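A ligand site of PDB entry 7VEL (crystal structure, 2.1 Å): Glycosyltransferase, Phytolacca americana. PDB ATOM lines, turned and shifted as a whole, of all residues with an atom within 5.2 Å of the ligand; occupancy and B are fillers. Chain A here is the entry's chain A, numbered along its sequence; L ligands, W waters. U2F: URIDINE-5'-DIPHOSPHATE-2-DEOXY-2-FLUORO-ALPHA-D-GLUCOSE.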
ATOM      1  N   HIS A  38     -22.461   7.097 -38.050  1.00  0.00           N
ATOM      2  CA  HIS A  38     -21.048   7.188 -37.709  1.00  0.00           C
ATOM      3  C   HIS A  38     -20.586   6.020 -36.843  1.00  0.00           C
ATOM      4  O   HIS A  38     -19.527   5.434 -37.081  1.00  0.00           O
ATOM      5  CB  HIS A  38     -20.788   8.524 -37.015  1.00  0.00           C
ATOM      6  CG  HIS A  38     -19.333   8.837 -36.832  1.00  0.00           C
ATOM      7  ND1 HIS A  38     -18.670   8.650 -35.635  1.00  0.00           N
ATOM      8  CD2 HIS A  38     -18.418   9.314 -37.703  1.00  0.00           C
ATOM      9  CE1 HIS A  38     -17.406   8.996 -35.775  1.00  0.00           C
ATOM     10  NE2 HIS A  38     -17.219   9.411 -37.017  1.00  0.00           N
ATOM     11  N   GLY A  39     -21.412   5.646 -35.851  1.00  0.00           N
ATOM     12  CA  GLY A  39     -21.089   4.567 -34.934  1.00  0.00           C
ATOM     13  C   GLY A  39     -21.022   3.185 -35.557  1.00  0.00           C
ATOM     14  O   GLY A  39     -20.476   2.265 -34.936  1.00  0.00           O
ATOM     15  N   HIS A  40     -21.594   3.006 -36.743  1.00  0.00           N
ATOM     16  CA  HIS A  40     -21.456   1.768 -37.485  1.00  0.00           C
ATOM     17  C   HIS A  40     -20.435   1.862 -38.589  1.00  0.00           C
ATOM     18  O   HIS A  40     -19.812   0.863 -38.956  1.00  0.00           O
ATOM     19  CB  HIS A  40     -22.791   1.365 -38.121  1.00  0.00           C
ATOM     20  CG  HIS A  40     -23.810   0.906 -37.132  1.00  0.00           C
ATOM     21  ND1 HIS A  40     -24.542  -0.258 -37.298  1.00  0.00           N
ATOM     22  CD2 HIS A  40     -24.218   1.432 -35.954  1.00  0.00           C
ATOM     23  CE1 HIS A  40     -25.351  -0.416 -36.266  1.00  0.00           C
ATOM     24  NE2 HIS A  40     -25.175   0.600 -35.435  1.00  0.00           N
ATOM     25  N   HIS A 165     -23.292  -5.949 -35.740  1.00  0.00           N
ATOM     26  CA  HIS A 165     -24.085  -5.047 -34.902  1.00  0.00           C
ATOM     27  C   HIS A 165     -23.288  -3.868 -34.350  1.00  0.00           C
ATOM     28  O   HIS A 165     -23.853  -2.775 -34.167  1.00  0.00           O
ATOM     29  CB  HIS A 165     -24.684  -5.769 -33.695  1.00  0.00           C
ATOM     30  CG  HIS A 165     -25.497  -6.977 -34.025  1.00  0.00           C
ATOM     31  ND1 HIS A 165     -24.930  -8.198 -34.349  1.00  0.00           N
ATOM     32  CD2 HIS A 165     -26.838  -7.180 -34.012  1.00  0.00           C
ATOM     33  CE1 HIS A 165     -25.891  -9.088 -34.543  1.00  0.00           C
ATOM     34  NE2 HIS A 165     -27.049  -8.495 -34.352  1.00  0.00           N
ATOM     35  N   GLY A 166     -22.019  -4.068 -33.985  1.00  0.00           N
ATOM     36  CA  GLY A 166     -21.252  -3.001 -33.378  1.00  0.00           C
ATOM     37  C   GLY A 166     -21.439  -2.810 -31.892  1.00  0.00           C
ATOM     38  O   GLY A 166     -21.136  -1.724 -31.385  1.00  0.00           O
ATOM     39  N   THR A 167     -21.913  -3.829 -31.174  1.00  0.00           N
ATOM     40  CA  THR A 167     -22.167  -3.730 -29.746  1.00  0.00           C
ATOM     41  C   THR A 167     -21.640  -4.987 -29.059  1.00  0.00           C
ATOM     42  O   THR A 167     -21.047  -5.869 -29.695  1.00  0.00           O
ATOM     43  CB  THR A 167     -23.666  -3.549 -29.449  1.00  0.00           C
ATOM     44  OG1 THR A 167     -23.852  -3.333 -28.040  1.00  0.00           O
ATOM     45  CG2 THR A 167     -24.437  -4.780 -29.876  1.00  0.00           C
ATOM     46  N   TYR A 307     -13.060  13.260 -18.154  1.00  0.00           N
ATOM     47  CA  TYR A 307     -13.418  13.537 -19.539  1.00  0.00           C
ATOM     48  C   TYR A 307     -14.903  13.287 -19.741  1.00  0.00           C
ATOM     49  O   TYR A 307     -15.417  12.218 -19.377  1.00  0.00           O
ATOM     50  CB  TYR A 307     -12.568  12.685 -20.487  1.00  0.00           C
ATOM     51  CG  TYR A 307     -12.926  12.763 -21.957  1.00  0.00           C
ATOM     52  CD1 TYR A 307     -12.594  13.879 -22.718  1.00  0.00           C
ATOM     53  CD2 TYR A 307     -13.533  11.696 -22.598  1.00  0.00           C
ATOM     54  CE1 TYR A 307     -12.902  13.939 -24.079  1.00  0.00           C
ATOM     55  CE2 TYR A 307     -13.835  11.741 -23.933  1.00  0.00           C
ATOM     56  CZ  TYR A 307     -13.526  12.853 -24.674  1.00  0.00           C
ATOM     57  OH  TYR A 307     -13.849  12.849 -26.020  1.00  0.00           O
ATOM     58  N   CYS A 309     -17.944  13.366 -22.625  1.00  0.00           N
ATOM     59  CA  CYS A 309     -18.294  13.433 -24.033  1.00  0.00           C
ATOM     60  C   CYS A 309     -19.437  12.472 -24.303  1.00  0.00           C
ATOM     61  O   CYS A 309     -19.431  11.338 -23.803  1.00  0.00           O
ATOM     62  CB  CYS A 309     -17.089  13.106 -24.916  1.00  0.00           C
ATOM     63  SG  CYS A 309     -17.320  13.439 -26.664  1.00  0.00           S
ATOM     64  N   GLY A 311     -20.695  11.248 -27.371  1.00  0.00           N
ATOM     65  CA  GLY A 311     -20.757  10.477 -28.596  1.00  0.00           C
ATOM     66  C   GLY A 311     -20.712  11.339 -29.852  1.00  0.00           C
ATOM     67  O   GLY A 311     -20.720  12.579 -29.801  1.00  0.00           O
ATOM     68  N   SER A 312     -20.647  10.646 -30.985  1.00  0.00           N
ATOM     69  CA  SER A 312     -20.459  11.323 -32.272  1.00  0.00           C
ATOM     70  C   SER A 312     -21.630  12.247 -32.584  1.00  0.00           C
ATOM     71  O   SER A 312     -21.433  13.347 -33.098  1.00  0.00           O
ATOM     72  CB  SER A 312     -20.286  10.292 -33.380  1.00  0.00           C
ATOM     73  OG  SER A 312     -21.310   9.306 -33.322  1.00  0.00           O
ATOM     74  N   THR A 313     -22.848  11.803 -32.281  1.00  0.00           N
ATOM     75  CA  THR A 313     -24.053  12.587 -32.496  1.00  0.00           C
ATOM     76  C   THR A 313     -24.741  12.793 -31.146  1.00  0.00           C
ATOM     77  O   THR A 313     -25.276  11.848 -30.570  1.00  0.00           O
ATOM     78  CB  THR A 313     -24.981  11.889 -33.487  1.00  0.00           C
ATOM     79  OG1 THR A 313     -26.338  12.299 -33.262  1.00  0.00           O
ATOM     80  CG2 THR A 313     -24.867  10.376 -33.360  1.00  0.00           C
ATOM     81  N   VAL A 338     -16.548  18.025 -23.661  1.00  0.00           N
ATOM     82  CA  VAL A 338     -16.789  18.129 -25.091  1.00  0.00           C
ATOM     83  C   VAL A 338     -18.259  18.473 -25.314  1.00  0.00           C
ATOM     84  O   VAL A 338     -19.147  17.699 -24.944  1.00  0.00           O
ATOM     85  CB  VAL A 338     -16.429  16.820 -25.806  1.00  0.00           C
ATOM     86  CG1 VAL A 338     -16.636  16.961 -27.327  1.00  0.00           C
ATOM     87  CG2 VAL A 338     -15.002  16.407 -25.480  1.00  0.00           C
ATOM     88  N   GLY A 371     -15.296  21.599 -30.676  1.00  0.00           N
ATOM     89  CA  GLY A 371     -15.174  20.821 -31.897  1.00  0.00           C
ATOM     90  C   GLY A 371     -15.130  19.333 -31.630  1.00  0.00           C
ATOM     91  O   GLY A 371     -15.509  18.844 -30.565  1.00  0.00           O
ATOM     92  N   TRP A 372     -14.644  18.605 -32.633  1.00  0.00           N
ATOM     93  CA  TRP A 372     -14.423  17.178 -32.519  1.00  0.00           C
ATOM     94  C   TRP A 372     -13.151  16.950 -31.707  1.00  0.00           C
ATOM     95  O   TRP A 372     -12.082  17.452 -32.066  1.00  0.00           O
ATOM     96  CB  TRP A 372     -14.297  16.564 -33.921  1.00  0.00           C
ATOM     97  CG  TRP A 372     -14.172  15.069 -34.008  1.00  0.00           C
ATOM     98  CD1 TRP A 372     -13.020  14.369 -34.223  1.00  0.00           C
ATOM     99  CD2 TRP A 372     -15.230  14.099 -33.931  1.00  0.00           C
ATOM    100  NE1 TRP A 372     -13.284  13.023 -34.281  1.00  0.00           N
ATOM    101  CE2 TRP A 372     -14.628  12.822 -34.104  1.00  0.00           C
ATOM    102  CE3 TRP A 372     -16.609  14.178 -33.735  1.00  0.00           C
ATOM    103  CZ2 TRP A 372     -15.380  11.645 -34.082  1.00  0.00           C
ATOM    104  CZ3 TRP A 372     -17.351  13.000 -33.708  1.00  0.00           C
ATOM    105  CH2 TRP A 372     -16.728  11.743 -33.875  1.00  0.00           C
ATOM    106  N   ALA A 373     -13.281  16.212 -30.586  1.00  0.00           N
ATOM    107  CA  ALA A 373     -12.146  16.019 -29.697  1.00  0.00           C
ATOM    108  C   ALA A 373     -11.368  14.749 -30.068  1.00  0.00           C
ATOM    109  O   ALA A 373     -11.945  13.793 -30.587  1.00  0.00           O
ATOM    110  CB  ALA A 373     -12.610  15.928 -28.254  1.00  0.00           C
ATOM    111  N   PRO A 374     -10.060  14.710 -29.804  1.00  0.00           N
ATOM    112  CA  PRO A 374      -9.290  13.464 -30.021  1.00  0.00           C
ATOM    113  C   PRO A 374      -9.503  12.512 -28.849  1.00  0.00           C
ATOM    114  O   PRO A 374      -8.700  12.436 -27.914  1.00  0.00           O
ATOM    115  CB  PRO A 374      -7.851  13.968 -30.119  1.00  0.00           C
ATOM    116  CG  PRO A 374      -7.834  15.183 -29.229  1.00  0.00           C
ATOM    117  CD  PRO A 374      -9.202  15.815 -29.347  1.00  0.00           C
ATOM    118  N   GLN A 375     -10.617  11.784 -28.880  1.00  0.00           N
ATOM    119  CA  GLN A 375     -11.084  11.079 -27.696  1.00  0.00           C
ATOM    120  C   GLN A 375     -10.088  10.015 -27.245  1.00  0.00           C
ATOM    121  O   GLN A 375      -9.847   9.849 -26.041  1.00  0.00           O
ATOM    122  CB  GLN A 375     -12.446  10.444 -27.944  1.00  0.00           C
ATOM    123  CG  GLN A 375     -12.960   9.628 -26.774  1.00  0.00           C
ATOM    124  CD  GLN A 375     -14.475   9.456 -26.778  1.00  0.00           C
ATOM    125  OE1 GLN A 375     -15.231  10.435 -26.720  1.00  0.00           O
ATOM    126  NE2 GLN A 375     -14.933   8.206 -26.829  1.00  0.00           N
ATOM    127  N   VAL A 376      -9.526   9.257 -28.184  1.00  0.00           N
ATOM    128  CA  VAL A 376      -8.604   8.188 -27.826  1.00  0.00           C
ATOM    129  C   VAL A 376      -7.322   8.757 -27.214  1.00  0.00           C
ATOM    130  O   VAL A 376      -6.872   8.314 -26.148  1.00  0.00           O
ATOM    131  CB  VAL A 376      -8.315   7.302 -29.050  1.00  0.00           C
ATOM    132  CG1 VAL A 376      -7.200   6.307 -28.751  1.00  0.00           C
ATOM    133  CG2 VAL A 376      -9.579   6.555 -29.460  1.00  0.00           C
ATOM    134  N   THR A 389     -19.900   9.154 -19.985  1.00  0.00           N
ATOM    135  CA  THR A 389     -20.207   8.673 -21.328  1.00  0.00           C
ATOM    136  C   THR A 389     -21.668   8.262 -21.415  1.00  0.00           C
ATOM    137  O   THR A 389     -22.337   8.028 -20.396  1.00  0.00           O
ATOM    138  CB  THR A 389     -19.311   7.493 -21.729  1.00  0.00           C
ATOM    139  OG1 THR A 389     -19.660   7.035 -23.035  1.00  0.00           O
ATOM    140  CG2 THR A 389     -19.459   6.340 -20.733  1.00  0.00           C
ATOM    141  N   HIS A 390     -22.184   8.193 -22.641  1.00  0.00           N
ATOM    142  CA  HIS A 390     -23.558   7.736 -22.863  1.00  0.00           C
ATOM    143  C   HIS A 390     -23.670   6.229 -23.024  1.00  0.00           C
ATOM    144  O   HIS A 390     -24.776   5.724 -23.234  1.00  0.00           O
ATOM    145  CB  HIS A 390     -24.160   8.427 -24.092  1.00  0.00           C
ATOM    146  CG  HIS A 390     -23.510   8.018 -25.387  1.00  0.00           C
ATOM    147  ND1 HIS A 390     -24.208   7.959 -26.579  1.00  0.00           N
ATOM    148  CD2 HIS A 390     -22.243   7.647 -25.671  1.00  0.00           C
ATOM    149  CE1 HIS A 390     -23.383   7.566 -27.539  1.00  0.00           C
ATOM    150  NE2 HIS A 390     -22.183   7.377 -27.013  1.00  0.00           N
ATOM    151  N   CYS A 391     -22.569   5.492 -22.922  1.00  0.00           N
ATOM    152  CA  CYS A 391     -22.525   4.035 -23.004  1.00  0.00           C
ATOM    153  C   CYS A 391     -22.790   3.493 -24.404  1.00  0.00           C
ATOM    154  O   CYS A 391     -23.188   2.332 -24.544  1.00  0.00           O
ATOM    155  CB  CYS A 391     -23.505   3.366 -22.030  1.00  0.00           C
ATOM    156  SG  CYS A 391     -23.244   3.836 -20.338  1.00  0.00           S
ATOM    157  N   GLY A 392     -22.609   4.310 -25.443  1.00  0.00           N
ATOM    158  CA  GLY A 392     -22.459   3.732 -26.764  1.00  0.00           C
ATOM    159  C   GLY A 392     -21.300   2.759 -26.754  1.00  0.00           C
ATOM    160  O   GLY A 392     -20.346   2.917 -25.980  1.00  0.00           O
ATOM    161  N   TRP A 393     -21.377   1.724 -27.576  1.00  0.00           N
ATOM    162  CA  TRP A 393     -20.379   0.665 -27.443  1.00  0.00           C
ATOM    163  C   TRP A 393     -18.997   1.120 -27.905  1.00  0.00           C
ATOM    164  O   TRP A 393     -17.997   0.656 -27.338  1.00  0.00           O
ATOM    165  CB  TRP A 393     -20.797  -0.602 -28.195  1.00  0.00           C
ATOM    166  CG  TRP A 393     -19.859  -1.769 -27.917  1.00  0.00           C
ATOM    167  CD1 TRP A 393     -19.155  -2.497 -28.836  1.00  0.00           C
ATOM    168  CD2 TRP A 393     -19.522  -2.333 -26.635  1.00  0.00           C
ATOM    169  NE1 TRP A 393     -18.407  -3.465 -28.209  1.00  0.00           N
ATOM    170  CE2 TRP A 393     -18.619  -3.383 -26.853  1.00  0.00           C
ATOM    171  CE3 TRP A 393     -19.895  -2.025 -25.310  1.00  0.00           C
ATOM    172  CZ2 TRP A 393     -18.079  -4.145 -25.804  1.00  0.00           C
ATOM    173  CZ3 TRP A 393     -19.359  -2.785 -24.275  1.00  0.00           C
ATOM    174  CH2 TRP A 393     -18.457  -3.838 -24.530  1.00  0.00           C
ATOM    175  N   ASN A 394     -18.899   2.000 -28.912  1.00  0.00           N
ATOM    176  CA  ASN A 394     -17.565   2.437 -29.335  1.00  0.00           C
ATOM    177  C   ASN A 394     -16.865   3.234 -28.239  1.00  0.00           C
ATOM    178  O   ASN A 394     -15.684   3.014 -27.943  1.00  0.00           O
ATOM    179  CB  ASN A 394     -17.656   3.251 -30.623  1.00  0.00           C
ATOM    180  CG  ASN A 394     -18.161   2.431 -31.795  1.00  0.00           C
ATOM    181  OD1 ASN A 394     -17.599   1.383 -32.125  1.00  0.00           O
ATOM    182  ND2 ASN A 394     -19.249   2.879 -32.394  1.00  0.00           N
ATOM    183  N   SER A 395     -17.595   4.140 -27.587  1.00  0.00           N
ATOM    184  CA  SER A 395     -16.995   4.870 -26.469  1.00  0.00           C
ATOM    185  C   SER A 395     -16.706   3.939 -25.296  1.00  0.00           C
ATOM    186  O   SER A 395     -15.677   4.087 -24.632  1.00  0.00           O
ATOM    187  CB  SER A 395     -17.890   6.011 -26.016  1.00  0.00           C
ATOM    188  OG  SER A 395     -17.725   7.129 -26.866  1.00  0.00           O
ATOM    189  N   GLU A 398     -13.612   2.093 -25.983  1.00  0.00           N
ATOM    190  CA  GLU A 398     -12.443   2.970 -25.867  1.00  0.00           C
ATOM    191  C   GLU A 398     -12.086   3.228 -24.405  1.00  0.00           C
ATOM    192  O   GLU A 398     -10.898   3.241 -24.049  1.00  0.00           O
ATOM    193  CB  GLU A 398     -12.696   4.274 -26.615  1.00  0.00           C
ATOM    194  CG  GLU A 398     -12.535   4.134 -28.108  1.00  0.00           C
ATOM    195  CD  GLU A 398     -13.113   5.313 -28.876  1.00  0.00           C
ATOM    196  OE1 GLU A 398     -13.614   6.266 -28.231  1.00  0.00           O
ATOM    197  OE2 GLU A 398     -13.040   5.301 -30.126  1.00  0.00           O
ATOM    198  N   PHE A 412     -30.530   5.939 -25.191  1.00  0.00           N
ATOM    199  CA  PHE A 412     -31.435   5.118 -26.002  1.00  0.00           C
ATOM    200  C   PHE A 412     -30.659   3.919 -26.539  1.00  0.00           C
ATOM    201  O   PHE A 412     -29.602   3.564 -26.012  1.00  0.00           O
ATOM    202  CB  PHE A 412     -32.116   5.976 -27.094  1.00  0.00           C
ATOM    203  CG  PHE A 412     -31.265   6.200 -28.325  1.00  0.00           C
ATOM    204  CD1 PHE A 412     -29.953   6.645 -28.215  1.00  0.00           C
ATOM    205  CD2 PHE A 412     -31.781   5.932 -29.577  1.00  0.00           C
ATOM    206  CE1 PHE A 412     -29.172   6.840 -29.352  1.00  0.00           C
ATOM    207  CE2 PHE A 412     -31.004   6.120 -30.729  1.00  0.00           C
ATOM    208  CZ  PHE A 412     -29.697   6.573 -30.609  1.00  0.00           C
ATOM    209  N   ALA A 413     -31.193   3.277 -27.576  1.00  0.00           N
ATOM    210  CA  ALA A 413     -30.583   2.137 -28.297  1.00  0.00           C
ATOM    211  C   ALA A 413     -30.307   1.021 -27.286  1.00  0.00           C
ATOM    212  O   ALA A 413     -31.187   0.687 -26.473  1.00  0.00           O
ATOM    213  CB  ALA A 413     -29.372   2.608 -29.097  1.00  0.00           C
ATOM    214  N   GLU A 414     -29.129   0.400 -27.316  1.00  0.00           N
ATOM    215  CA  GLU A 414     -28.806  -0.688 -26.401  1.00  0.00           C
ATOM    216  C   GLU A 414     -27.986  -0.212 -25.198  1.00  0.00           C
ATOM    217  O   GLU A 414     -27.394  -1.026 -24.482  1.00  0.00           O
ATOM    218  CB  GLU A 414     -28.083  -1.817 -27.170  1.00  0.00           C
ATOM    219  CG  GLU A 414     -26.538  -1.800 -27.201  1.00  0.00           C
ATOM    220  CD  GLU A 414     -25.915  -0.629 -27.953  1.00  0.00           C
ATOM    221  OE1 GLU A 414     -26.613   0.353 -28.250  1.00  0.00           O
ATOM    222  OE2 GLU A 414     -24.699  -0.705 -28.248  1.00  0.00           O
ATOM    223  N   GLN A 415     -28.007   1.103 -24.939  1.00  0.00           N
ATOM    224  CA  GLN A 415     -27.085   1.693 -23.972  1.00  0.00           C
ATOM    225  C   GLN A 415     -27.399   1.292 -22.532  1.00  0.00           C
ATOM    226  O   GLN A 415     -26.498   1.245 -21.698  1.00  0.00           O
ATOM    227  CB  GLN A 415     -27.083   3.215 -24.135  1.00  0.00           C
ATOM    228  CG  GLN A 415     -26.390   3.662 -25.442  1.00  0.00           C
ATOM    229  CD  GLN A 415     -26.857   5.046 -25.916  1.00  0.00           C
ATOM    230  OE1 GLN A 415     -27.372   5.841 -25.130  1.00  0.00           O
ATOM    231  NE2 GLN A 415     -26.711   5.317 -27.209  1.00  0.00           N
ATOM    232  N   ASN A 418     -25.613  -1.912 -22.064  1.00  0.00           N
ATOM    233  CA  ASN A 418     -24.195  -1.614 -21.918  1.00  0.00           C
ATOM    234  C   ASN A 418     -23.885  -1.082 -20.516  1.00  0.00           C
ATOM    235  O   ASN A 418     -22.846  -1.406 -19.935  1.00  0.00           O
ATOM    236  CB  ASN A 418     -23.740  -0.615 -22.982  1.00  0.00           C
ATOM    237  CG  ASN A 418     -23.704  -1.210 -24.387  1.00  0.00           C
ATOM    238  OD1 ASN A 418     -23.707  -2.437 -24.573  1.00  0.00           O
ATOM    239  ND2 ASN A 418     -23.642  -0.341 -25.394  1.00  0.00           N
HETATM  240  C1  U2F L   1     -24.166   4.640 -31.610  1.00  0.00           C
HETATM  241  O1  U2F L   1     -23.262   5.199 -30.755  1.00  0.00           O
HETATM  242  PB  U2F L   1     -22.236   6.386 -31.319  1.00  0.00           P
HETATM  243  O1B U2F L   1     -22.931   7.437 -32.123  1.00  0.00           O
HETATM  244  O2B U2F L   1     -21.118   5.744 -32.100  1.00  0.00           O
HETATM  245  O3A U2F L   1     -21.514   7.007 -29.970  1.00  0.00           O
HETATM  246  PA  U2F L   1     -20.227   6.166 -29.311  1.00  0.00           P
HETATM  247  O1A U2F L   1     -20.462   4.680 -29.260  1.00  0.00           O
HETATM  248  O2A U2F L   1     -20.005   6.750 -27.930  1.00  0.00           O
HETATM  249  O5' U2F L   1     -18.932   6.408 -30.305  1.00  0.00           O
HETATM  250  C5' U2F L   1     -18.324   7.687 -30.287  1.00  0.00           C
HETATM  251  C4' U2F L   1     -17.118   7.539 -31.207  1.00  0.00           C
HETATM  252  O4' U2F L   1     -16.780   8.976 -31.833  1.00  0.00           O
HETATM  253  C1' U2F L   1     -15.621   9.333 -31.358  1.00  0.00           C
HETATM  254  C2' U2F L   1     -15.266   8.369 -30.223  1.00  0.00           C
HETATM  255  C3' U2F L   1     -16.084   7.110 -30.553  1.00  0.00           C
HETATM  256  O3' U2F L   1     -15.252   6.236 -31.433  1.00  0.00           O
HETATM  257  O2' U2F L   1     -13.930   8.035 -30.304  1.00  0.00           O
HETATM  258  N1  U2F L   1     -15.683  10.767 -30.913  1.00  0.00           N
HETATM  259  C6' U2F L   1     -14.434  11.563 -31.024  1.00  0.00           C
HETATM  260  O6' U2F L   1     -13.457  11.046 -31.429  1.00  0.00           O
HETATM  261  N3  U2F L   1     -14.445  13.003 -30.605  1.00  0.00           N
HETATM  262  C7' U2F L   1     -15.662  13.612 -30.115  1.00  0.00           C
HETATM  263  O7' U2F L   1     -15.655  14.764 -29.788  1.00  0.00           O
HETATM  264  C8' U2F L   1     -16.915  12.798 -30.022  1.00  0.00           C
HETATM  265  C9' U2F L   1     -16.909  11.367 -30.430  1.00  0.00           C
HETATM  266  C2  U2F L   1     -25.306   4.167 -30.732  1.00  0.00           C
HETATM  267  F1  U2F L   1     -25.802   5.287 -30.052  1.00  0.00           F
HETATM  268  C3  U2F L   1     -24.758   3.230 -29.723  1.00  0.00           C
HETATM  269  O3  U2F L   1     -25.860   2.835 -28.878  1.00  0.00           O
HETATM  270  C4  U2F L   1     -24.125   2.017 -30.373  1.00  0.00           C
HETATM  271  O4  U2F L   1     -23.568   1.141 -29.370  1.00  0.00           O
HETATM  272  C5  U2F L   1     -23.039   2.456 -31.361  1.00  0.00           C
HETATM  273  C6  U2F L   1     -22.548   1.253 -32.143  1.00  0.00           C
HETATM  274  O6  U2F L   1     -23.648   0.444 -32.465  1.00  0.00           O
HETATM  275  O5  U2F L   1     -23.526   3.485 -32.304  1.00  0.00           O
HETATM  276  O   HOH W   1     -23.415   6.785 -34.825  1.00  0.00           O
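O of His 390 lies close to OE1 of Gln 415 (3.2 Å). NE2 of His 390 sits close to N of Gly 392 (3.5 Å). The side-chain amide oxygen of Gln 375 sits at hydrogen-bond distance from the side-chain sulfur of Cys 309 (3.7 Å). OE1 of Gln 415 lies within hydrogen-bond range of N of Phe 412 (3.2 Å). OG of Ser 395 lies within hydrogen-bond range of NE2 of Gln 375, 3.0 Å away. The side-chain amide nitrogen (NE2) of Gln 375 lies within hydrogen-bond range of the side-chain carboxylate (OE1) of Glu 398. The side-chain carboxylate of Glu 414 lies within hydrogen-bond range of the side-chain amide nitrogen of Asn 418 (3.1 Å). OE2 of Glu 414 sits at hydrogen-bond distance from OG1 of Thr 167, at 2.8 Å.
Water W1 lies within hydrogen-bond range of N of Gly 39 (2.5 Å), O1B of the ligand (2.8 Å) and N of His 38 (3.4 Å).
Merely in contact with the ligand: Gly 39 (3.1 Å), Gly 392 (3.3 Å), Gln 375 (3.4 Å), Val 338 (3.4 Å), Ala 413 (3.5 Å), His 165 (3.6 Å), Thr 313 (3.7 Å), Phe 412 (3.8 Å), Gly 311 (3.8 Å) and His 38 (3.99 Å). Hydrophobic or aromatic side chains within 4 Å of the ligand: His 38, His 40, Val 338, Trp 372, Ala 373, His 390, Trp 393, Phe 412 and Ala 413. Of the 31 residues printed, 23 come within 4 Å of the ligand. The nearest printed residue that does not touch the ligand is Gly 371 (4.2 Å).
O7' of the ligand sits close to SG of Cys 309, 3.8 Å away. OE2 of Glu 398 sits at hydrogen-bond distance from O3' of the ligand, 2.7 Å away. O of Ala 373 is in hydrogen-bond range of N3 of the ligand (2.6 Å). An oxygen (O6') of the ligand lies close to the indole nitrogen of Trp 372, at 3.5 Å. O7' of the ligand lies within hydrogen-bond range of N of Ala 373 (2.9 Å). ND2 of Asn 394 lies within hydrogen-bond range of O2B of the ligand, at 3.4 Å. O3 of the ligand lies within hydrogen-bond range of NE2 of Gln 415, at 3.1 Å. O2A of the ligand sits at hydrogen-bond distance from OG of Ser 395 (2.5 Å). The backbone carbonyl oxygen of Gly 166 lies close to an oxygen (O6) of the ligand (3.5 Å). The backbone NH (N) of Asn 394 lies within hydrogen-bond range of an oxygen (O1A) of the ligand (3.1 Å). The side-chain hydroxyl of Ser 312 is in hydrogen-bond range of an oxygen (O1B) of the ligand (2.7 Å). NE2 of His 40 sits at hydrogen-bond distance from O6 of the ligand (3.3 Å). OE2 of Glu 414 is in hydrogen-bond range of O4 of the ligand. A ring nitrogen (NE2) of His 390 is in hydrogen-bond range of an oxygen (O2A) of the ligand (2.4 Å). O4 of the ligand is in hydrogen-bond range of N of Trp 393. The backbone NH of Ser 395 lies within hydrogen-bond range of an oxygen (O1A) of the ligand (3.4 Å).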
